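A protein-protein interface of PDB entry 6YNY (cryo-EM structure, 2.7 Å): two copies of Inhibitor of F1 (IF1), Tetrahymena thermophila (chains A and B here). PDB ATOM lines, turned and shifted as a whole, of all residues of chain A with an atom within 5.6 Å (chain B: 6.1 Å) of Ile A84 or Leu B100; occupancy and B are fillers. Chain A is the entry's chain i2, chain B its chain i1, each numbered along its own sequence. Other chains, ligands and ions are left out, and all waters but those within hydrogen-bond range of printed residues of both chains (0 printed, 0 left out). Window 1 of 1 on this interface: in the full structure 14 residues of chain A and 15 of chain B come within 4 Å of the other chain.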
ATOM      1  N   GLU A  80      22.172  15.896  -6.180  1.00  0.00           N
ATOM      2  CA  GLU A  80      20.712  16.147  -6.067  1.00  0.00           C
ATOM      3  C   GLU A  80      19.951  15.120  -6.914  1.00  0.00           C
ATOM      4  O   GLU A  80      18.973  14.541  -6.402  1.00  0.00           O
ATOM      5  CB  GLU A  80      20.381  17.573  -6.512  1.00  0.00           C
ATOM      6  CG  GLU A  80      20.268  18.557  -5.361  1.00  0.00           C
ATOM      7  CD  GLU A  80      20.326  20.019  -5.771  1.00  0.00           C
ATOM      8  OE1 GLU A  80      19.803  20.349  -6.853  1.00  0.00           O
ATOM      9  OE2 GLU A  80      20.895  20.822  -5.006  1.00  0.00           O
ATOM     10  N   VAL A  81      20.391  14.910  -8.159  1.00  0.00           N
ATOM     11  CA  VAL A  81      19.777  13.972  -9.093  1.00  0.00           C
ATOM     12  C   VAL A  81      19.848  12.554  -8.553  1.00  0.00           C
ATOM     13  O   VAL A  81      18.983  11.722  -8.852  1.00  0.00           O
ATOM     14  CB  VAL A  81      20.452  14.073 -10.472  1.00  0.00           C
ATOM     15  CG1 VAL A  81      19.857  13.061 -11.429  1.00  0.00           C
ATOM     16  CG2 VAL A  81      20.311  15.471 -11.016  1.00  0.00           C
ATOM     17  N   GLU A  82      20.899  12.274  -7.778  1.00  0.00           N
ATOM     18  CA  GLU A  82      21.152  10.948  -7.152  1.00  0.00           C
ATOM     19  C   GLU A  82      20.054  10.613  -6.135  1.00  0.00           C
ATOM     20  O   GLU A  82      19.601   9.451  -6.129  1.00  0.00           O
ATOM     21  CB  GLU A  82      22.525  10.937  -6.478  1.00  0.00           C
ATOM     22  CG  GLU A  82      23.292   9.644  -6.689  1.00  0.00           C
ATOM     23  CD  GLU A  82      24.787   9.821  -6.888  1.00  0.00           C
ATOM     24  OE1 GLU A  82      25.323  10.855  -6.442  1.00  0.00           O
ATOM     25  OE2 GLU A  82      25.413   8.924  -7.488  1.00  0.00           O
ATOM     26  N   ASN A  83      19.642  11.584  -5.311  1.00  0.00           N
ATOM     27  CA  ASN A  83      18.638  11.378  -4.272  1.00  0.00           C
ATOM     28  C   ASN A  83      17.238  11.292  -4.866  1.00  0.00           C
ATOM     29  O   ASN A  83      16.451  10.410  -4.503  1.00  0.00           O
ATOM     30  CB  ASN A  83      18.714  12.502  -3.239  1.00  0.00           C
ATOM     31  CG  ASN A  83      20.040  12.534  -2.511  1.00  0.00           C
ATOM     32  OD1 ASN A  83      20.725  11.517  -2.401  1.00  0.00           O
ATOM     33  ND2 ASN A  83      20.407  13.703  -2.003  1.00  0.00           N
ATOM     34  N   ILE A  84      16.906  12.208  -5.777  1.00  0.00           N
ATOM     35  CA  ILE A  84      15.557  12.246  -6.338  1.00  0.00           C
ATOM     36  C   ILE A  84      15.233  10.935  -7.042  1.00  0.00           C
ATOM     37  O   ILE A  84      14.124  10.401  -6.912  1.00  0.00           O
ATOM     38  CB  ILE A  84      15.408  13.452  -7.284  1.00  0.00           C
ATOM     39  CG1 ILE A  84      13.980  13.538  -7.814  1.00  0.00           C
ATOM     40  CG2 ILE A  84      16.368  13.338  -8.443  1.00  0.00           C
ATOM     41  CD1 ILE A  84      13.683  14.831  -8.528  1.00  0.00           C
ATOM     42  N   LEU A  85      16.186  10.395  -7.802  1.00  0.00           N
ATOM     43  CA  LEU A  85      15.939   9.140  -8.503  1.00  0.00           C
ATOM     44  C   LEU A  85      15.813   7.981  -7.524  1.00  0.00           C
ATOM     45  O   LEU A  85      15.004   7.070  -7.732  1.00  0.00           O
ATOM     46  CB  LEU A  85      17.053   8.869  -9.511  1.00  0.00           C
ATOM     47  CG  LEU A  85      17.119   9.815 -10.709  1.00  0.00           C
ATOM     48  CD1 LEU A  85      18.354   9.538 -11.538  1.00  0.00           C
ATOM     49  CD2 LEU A  85      15.873   9.686 -11.563  1.00  0.00           C
ATOM     50  N   LYS A  86      16.607   7.996  -6.451  1.00  0.00           N
ATOM     51  CA  LYS A  86      16.519   6.931  -5.460  1.00  0.00           C
ATOM     52  C   LYS A  86      15.147   6.899  -4.802  1.00  0.00           C
ATOM     53  O   LYS A  86      14.669   5.827  -4.419  1.00  0.00           O
ATOM     54  CB  LYS A  86      17.616   7.108  -4.411  1.00  0.00           C
ATOM     55  CG  LYS A  86      18.998   6.716  -4.906  1.00  0.00           C
ATOM     56  CD  LYS A  86      20.059   6.844  -3.823  1.00  0.00           C
ATOM     57  CE  LYS A  86      20.228   8.282  -3.372  1.00  0.00           C
ATOM     58  NZ  LYS A  86      21.383   8.448  -2.449  1.00  0.00           N
ATOM     59  N   ARG A  87      14.502   8.059  -4.661  1.00  0.00           N
ATOM     60  CA  ARG A  87      13.165   8.092  -4.080  1.00  0.00           C
ATOM     61  C   ARG A  87      12.191   7.259  -4.898  1.00  0.00           C
ATOM     62  O   ARG A  87      11.328   6.572  -4.342  1.00  0.00           O
ATOM     63  CB  ARG A  87      12.665   9.529  -3.970  1.00  0.00           C
ATOM     64  CG  ARG A  87      13.486  10.400  -3.057  1.00  0.00           C
ATOM     65  CD  ARG A  87      12.611  11.442  -2.412  1.00  0.00           C
ATOM     66  NE  ARG A  87      11.785  12.141  -3.390  1.00  0.00           N
ATOM     67  CZ  ARG A  87      12.134  13.266  -4.003  1.00  0.00           C
ATOM     68  NH1 ARG A  87      11.309  13.819  -4.877  1.00  0.00           N
ATOM     69  NH2 ARG A  87      13.301  13.842  -3.744  1.00  0.00           N
ATOM     70  N   TYR A  88      12.307   7.317  -6.220  1.00  0.00           N
ATOM     71  CA  TYR A  88      11.460   6.533  -7.105  1.00  0.00           C
ATOM     72  C   TYR A  88      11.984   5.121  -7.315  1.00  0.00           C
ATOM     73  O   TYR A  88      11.471   4.411  -8.186  1.00  0.00           O
ATOM     74  CB  TYR A  88      11.309   7.251  -8.446  1.00  0.00           C
ATOM     75  CG  TYR A  88      10.464   8.496  -8.352  1.00  0.00           C
ATOM     76  CD1 TYR A  88       9.160   8.507  -8.819  1.00  0.00           C
ATOM     77  CD2 TYR A  88      10.962   9.654  -7.777  1.00  0.00           C
ATOM     78  CE1 TYR A  88       8.381   9.637  -8.726  1.00  0.00           C
ATOM     79  CE2 TYR A  88      10.189  10.789  -7.678  1.00  0.00           C
ATOM     80  CZ  TYR A  88       8.899  10.775  -8.153  1.00  0.00           C
ATOM     81  OH  TYR A  88       8.131  11.908  -8.055  1.00  0.00           O
ATOM     82  N   LEU A 100      21.636  14.391 -17.264  1.00  0.00           N
ATOM     83  CA  LEU A 100      20.728  15.242 -16.505  1.00  0.00           C
ATOM     84  C   LEU A 100      21.457  16.452 -15.937  1.00  0.00           C
ATOM     85  O   LEU A 100      20.940  17.575 -15.980  1.00  0.00           O
ATOM     86  CB  LEU A 100      20.071  14.437 -15.387  1.00  0.00           C
ATOM     87  CG  LEU A 100      19.233  13.243 -15.841  1.00  0.00           C
ATOM     88  CD1 LEU A 100      18.746  12.450 -14.647  1.00  0.00           C
ATOM     89  CD2 LEU A 100      18.060  13.702 -16.681  1.00  0.00           C
ATOM     90  N   TRP A 103      22.141  18.594 -18.799  1.00  0.00           N
ATOM     91  CA  TRP A 103      20.897  19.195 -19.265  1.00  0.00           C
ATOM     92  C   TRP A 103      20.532  20.420 -18.437  1.00  0.00           C
ATOM     93  O   TRP A 103      20.030  21.414 -18.973  1.00  0.00           O
ATOM     94  CB  TRP A 103      19.774  18.160 -19.220  1.00  0.00           C
ATOM     95  CG  TRP A 103      18.410  18.744 -19.373  1.00  0.00           C
ATOM     96  CD1 TRP A 103      17.845  19.220 -20.518  1.00  0.00           C
ATOM     97  CD2 TRP A 103      17.428  18.904 -18.344  1.00  0.00           C
ATOM     98  NE1 TRP A 103      16.573  19.673 -20.266  1.00  0.00           N
ATOM     99  CE2 TRP A 103      16.293  19.489 -18.938  1.00  0.00           C
ATOM    100  CE3 TRP A 103      17.399  18.612 -16.979  1.00  0.00           C
ATOM    101  CZ2 TRP A 103      15.143  19.788 -18.213  1.00  0.00           C
ATOM    102  CZ3 TRP A 103      16.257  18.907 -16.261  1.00  0.00           C
ATOM    103  CH2 TRP A 103      15.145  19.490 -16.878  1.00  0.00           C
ATOM    104  N   VAL B  81      13.478  16.101 -20.970  1.00  0.00           N
ATOM    105  CA  VAL B  81      13.802  15.066 -19.996  1.00  0.00           C
ATOM    106  C   VAL B  81      13.197  13.734 -20.413  1.00  0.00           C
ATOM    107  O   VAL B  81      13.827  12.679 -20.271  1.00  0.00           O
ATOM    108  CB  VAL B  81      13.327  15.489 -18.597  1.00  0.00           C
ATOM    109  CG1 VAL B  81      13.697  14.437 -17.570  1.00  0.00           C
ATOM    110  CG2 VAL B  81      13.917  16.835 -18.224  1.00  0.00           C
ATOM    111  N   LEU B  85      14.961   9.908 -20.832  1.00  0.00           N
ATOM    112  CA  LEU B  85      14.540   8.670 -20.188  1.00  0.00           C
ATOM    113  C   LEU B  85      14.205   7.604 -21.222  1.00  0.00           C
ATOM    114  O   LEU B  85      14.326   6.406 -20.941  1.00  0.00           O
ATOM    115  CB  LEU B  85      13.341   8.941 -19.279  1.00  0.00           C
ATOM    116  CG  LEU B  85      13.572  10.013 -18.209  1.00  0.00           C
ATOM    117  CD1 LEU B  85      12.277  10.372 -17.511  1.00  0.00           C
ATOM    118  CD2 LEU B  85      14.600   9.550 -17.197  1.00  0.00           C
ATOM    119  N   ALA B  95       5.189  12.531 -12.268  1.00  0.00           N
ATOM    120  CA  ALA B  95       5.685  13.086 -11.015  1.00  0.00           C
ATOM    121  C   ALA B  95       7.196  13.256 -11.060  1.00  0.00           C
ATOM    122  O   ALA B  95       7.730  14.299 -10.668  1.00  0.00           O
ATOM    123  CB  ALA B  95       5.279  12.189  -9.849  1.00  0.00           C
ATOM    124  N   LEU B  96       7.905  12.234 -11.539  1.00  0.00           N
ATOM    125  CA  LEU B  96       9.355  12.331 -11.657  1.00  0.00           C
ATOM    126  C   LEU B  96       9.747  13.459 -12.600  1.00  0.00           C
ATOM    127  O   LEU B  96      10.640  14.258 -12.297  1.00  0.00           O
ATOM    128  CB  LEU B  96       9.929  11.004 -12.149  1.00  0.00           C
ATOM    129  CG  LEU B  96      11.431  11.001 -12.419  1.00  0.00           C
ATOM    130  CD1 LEU B  96      12.197  11.424 -11.185  1.00  0.00           C
ATOM    131  CD2 LEU B  96      11.882   9.638 -12.882  1.00  0.00           C
ATOM    132  N   ILE B  97       9.084  13.539 -13.753  1.00  0.00           N
ATOM    133  CA  ILE B  97       9.404  14.579 -14.721  1.00  0.00           C
ATOM    134  C   ILE B  97       9.122  15.953 -14.133  1.00  0.00           C
ATOM    135  O   ILE B  97       9.901  16.895 -14.314  1.00  0.00           O
ATOM    136  CB  ILE B  97       8.619  14.349 -16.022  1.00  0.00           C
ATOM    137  CG1 ILE B  97       9.041  13.025 -16.665  1.00  0.00           C
ATOM    138  CG2 ILE B  97       8.836  15.508 -16.970  1.00  0.00           C
ATOM    139  CD1 ILE B  97       8.142  12.570 -17.791  1.00  0.00           C
ATOM    140  N   ASP B  98       8.009  16.088 -13.413  1.00  0.00           N
ATOM    141  CA  ASP B  98       7.678  17.372 -12.809  1.00  0.00           C
ATOM    142  C   ASP B  98       8.736  17.794 -11.801  1.00  0.00           C
ATOM    143  O   ASP B  98       9.094  18.975 -11.722  1.00  0.00           O
ATOM    144  CB  ASP B  98       6.305  17.299 -12.145  1.00  0.00           C
ATOM    145  CG  ASP B  98       5.187  17.065 -13.141  1.00  0.00           C
ATOM    146  OD1 ASP B  98       5.481  16.945 -14.349  1.00  0.00           O
ATOM    147  OD2 ASP B  98       4.015  17.001 -12.718  1.00  0.00           O
ATOM    148  N   GLU B  99       9.254  16.845 -11.020  1.00  0.00           N
ATOM    149  CA  GLU B  99      10.270  17.183 -10.029  1.00  0.00           C
ATOM    150  C   GLU B  99      11.584  17.558 -10.699  1.00  0.00           C
ATOM    151  O   GLU B  99      12.215  18.557 -10.332  1.00  0.00           O
ATOM    152  CB  GLU B  99      10.475  16.015  -9.068  1.00  0.00           C
ATOM    153  CG  GLU B  99       9.290  15.738  -8.165  1.00  0.00           C
ATOM    154  CD  GLU B  99       9.573  14.641  -7.162  1.00  0.00           C
ATOM    155  OE1 GLU B  99      10.755  14.271  -7.003  1.00  0.00           O
ATOM    156  OE2 GLU B  99       8.616  14.145  -6.533  1.00  0.00           O
ATOM    157  N   LEU B 100      12.015  16.769 -11.685  1.00  0.00           N
ATOM    158  CA  LEU B 100      13.234  17.108 -12.412  1.00  0.00           C
ATOM    159  C   LEU B 100      13.111  18.471 -13.077  1.00  0.00           C
ATOM    160  O   LEU B 100      14.049  19.276 -13.040  1.00  0.00           O
ATOM    161  CB  LEU B 100      13.546  16.031 -13.448  1.00  0.00           C
ATOM    162  CG  LEU B 100      13.970  14.671 -12.898  1.00  0.00           C
ATOM    163  CD1 LEU B 100      14.124  13.673 -14.023  1.00  0.00           C
ATOM    164  CD2 LEU B 100      15.261  14.786 -12.116  1.00  0.00           C
ATOM    165  N   VAL B 101      11.959  18.750 -13.687  1.00  0.00           N
ATOM    166  CA  VAL B 101      11.731  20.071 -14.261  1.00  0.00           C
ATOM    167  C   VAL B 101      11.812  21.137 -13.179  1.00  0.00           C
ATOM    168  O   VAL B 101      12.412  22.199 -13.377  1.00  0.00           O
ATOM    169  CB  VAL B 101      10.378  20.108 -14.994  1.00  0.00           C
ATOM    170  CG1 VAL B 101      10.005  21.534 -15.339  1.00  0.00           C
ATOM    171  CG2 VAL B 101      10.434  19.258 -16.249  1.00  0.00           C
ATOM    172  N   ASP B 102      11.214  20.871 -12.015  1.00  0.00           N
ATOM    173  CA  ASP B 102      11.330  21.813 -10.911  1.00  0.00           C
ATOM    174  C   ASP B 102      12.754  21.860 -10.378  1.00  0.00           C
ATOM    175  O   ASP B 102      13.199  22.902  -9.885  1.00  0.00           O
ATOM    176  CB  ASP B 102      10.360  21.435  -9.791  1.00  0.00           C
ATOM    177  CG  ASP B 102       8.912  21.448 -10.243  1.00  0.00           C
ATOM    178  OD1 ASP B 102       8.664  21.696 -11.441  1.00  0.00           O
ATOM    179  OD2 ASP B 102       8.024  21.208  -9.399  1.00  0.00           O
ATOM    180  N   TRP B 103      13.477  20.744 -10.466  1.00  0.00           N
ATOM    181  CA  TRP B 103      14.871  20.728 -10.037  1.00  0.00           C
ATOM    182  C   TRP B 103      15.735  21.589 -10.945  1.00  0.00           C
ATOM    183  O   TRP B 103      16.682  22.237 -10.483  1.00  0.00           O
ATOM    184  CB  TRP B 103      15.388  19.292 -10.011  1.00  0.00           C
ATOM    185  CG  TRP B 103      16.863  19.199  -9.857  1.00  0.00           C
ATOM    186  CD1 TRP B 103      17.582  19.401  -8.720  1.00  0.00           C
ATOM    187  CD2 TRP B 103      17.809  18.881 -10.880  1.00  0.00           C
ATOM    188  NE1 TRP B 103      18.920  19.229  -8.969  1.00  0.00           N
ATOM    189  CE2 TRP B 103      19.086  18.907 -10.290  1.00  0.00           C
ATOM    190  CE3 TRP B 103      17.701  18.574 -12.239  1.00  0.00           C
ATOM    191  CZ2 TRP B 103      20.245  18.643 -11.010  1.00  0.00           C
ATOM    192  CZ3 TRP B 103      18.851  18.309 -12.952  1.00  0.00           C
ATOM    193  CH2 TRP B 103      20.107  18.345 -12.338  1.00  0.00           C
ATOM    194  N   LYS B 104      15.427  21.606 -12.243  1.00  0.00           N
ATOM    195  CA  LYS B 104      16.180  22.439 -13.174  1.00  0.00           C
ATOM    196  C   LYS B 104      15.979  23.915 -12.863  1.00  0.00           C
ATOM    197  O   LYS B 104      16.939  24.694 -12.836  1.00  0.00           O
ATOM    198  CB  LYS B 104      15.760  22.119 -14.609  1.00  0.00           C
ATOM    199  CG  LYS B 104      16.635  22.742 -15.686  1.00  0.00           C
ATOM    200  CD  LYS B 104      16.197  24.153 -16.043  1.00  0.00           C
ATOM    201  CE  LYS B 104      16.929  24.663 -17.274  1.00  0.00           C
ATOM    202  NZ  LYS B 104      16.566  26.071 -17.596  1.00  0.00           N
ATOM    203  N   THR B 105      14.730  24.319 -12.625  1.00  0.00           N
ATOM    204  CA  THR B 105      14.454  25.714 -12.303  1.00  0.00           C
ATOM    205  C   THR B 105      15.032  26.099 -10.949  1.00  0.00           C
ATOM    206  O   THR B 105      15.458  27.243 -10.760  1.00  0.00           O
ATOM    207  CB  THR B 105      12.948  25.967 -12.326  1.00  0.00           C
ATOM    208  OG1 THR B 105      12.315  25.190 -11.301  1.00  0.00           O
ATOM    209  CG2 THR B 105      12.366  25.585 -13.679  1.00  0.00           C
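The side-chain carboxylate (OE1) of Glu A80 sits at hydrogen-bond distance from the indole nitrogen (NE1) of Trp B103.
The guanidinium group (NH1) of Arg A87 is in salt-bridge range of the side-chain carboxylate (OE2) of Glu B99, 3.2 Å away.
OE2 of Glu B99 lies within hydrogen-bond range of OH of Tyr A88.
Val A81 touches Trp B103, and with the chains exchanged Trp A103 touches Val B81.
Leu A100 touches Trp B103, and with the chains exchanged Trp A103 touches Leu B100.
4 positions are printed for both chains.
Of the 12 pairs that touch across the chains among the printed residues, 4 have their exchanged pair printed and touching as well.
Hydrophobic or aromatic side chains of chain B within 4 Å of the printed part of chain A: Val B81, Ala B95, Leu B96, Leu B100 and Trp B103.
Of the 11 printed residues of chain A, 7 touch a printed residue of chain B.
Hydrophobic or aromatic side chains of chain A within 4 Å of the printed part of chain B: Val A81, Ile A84, Tyr A88 and Trp A103.
Along chain A the printed residues that touch a printed residue of chain B span positions 80 to 103.
Among the printed residues, pairs that only touch across the chains: Val A81 with Trp B103 (3.2 Å), Ile A84 with Glu B99 (3.3 Å), Ile A84 with Leu B100 (3.9 Å), Tyr A88 with Ala B95 (3.4 Å), Tyr A88 with Leu B96 (3.5 Å), Leu A100 with Trp B103 (3.8 Å), Trp A103 with Val B81 (3.2 Å), Trp A103 with Leu B100 (3.9 Å) and Trp A103 with Lys B104 (3.5 Å).
Of the printed residues of chain B, Glu A80 touches Trp B103 (2.6 Å).
Ile A84 touches two residues of chain B.
Of the printed residues of chain B, Tyr A88 touches Ala B95 (3.4 Å), Leu B96 (3.5 Å) and Glu B99 (2.7 Å).
Of the printed residues of chain A, Val B81 touches Trp A103.
Printed residues of chain A within 4 Å of Glu B99: Ile A84 (3.3 Å), Arg A87 (2.2 Å) and Tyr A88 (2.7 Å).
Of the printed residues of chain A, Leu B100 touches Ile A84 and Trp A103.
Of the printed residues of chain A, Lys B104 touches Trp A103 (3.5 Å).
The nearest residue of chain B that does not touch Ile A84 is Leu B96 (4.4 Å).
The nearest residue of chain A that does not touch Leu B100 is Leu A100 (4.7 Å).
The nearest printed residue of chain A that does not touch Lys B104 is Leu A100 (6.7 Å).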
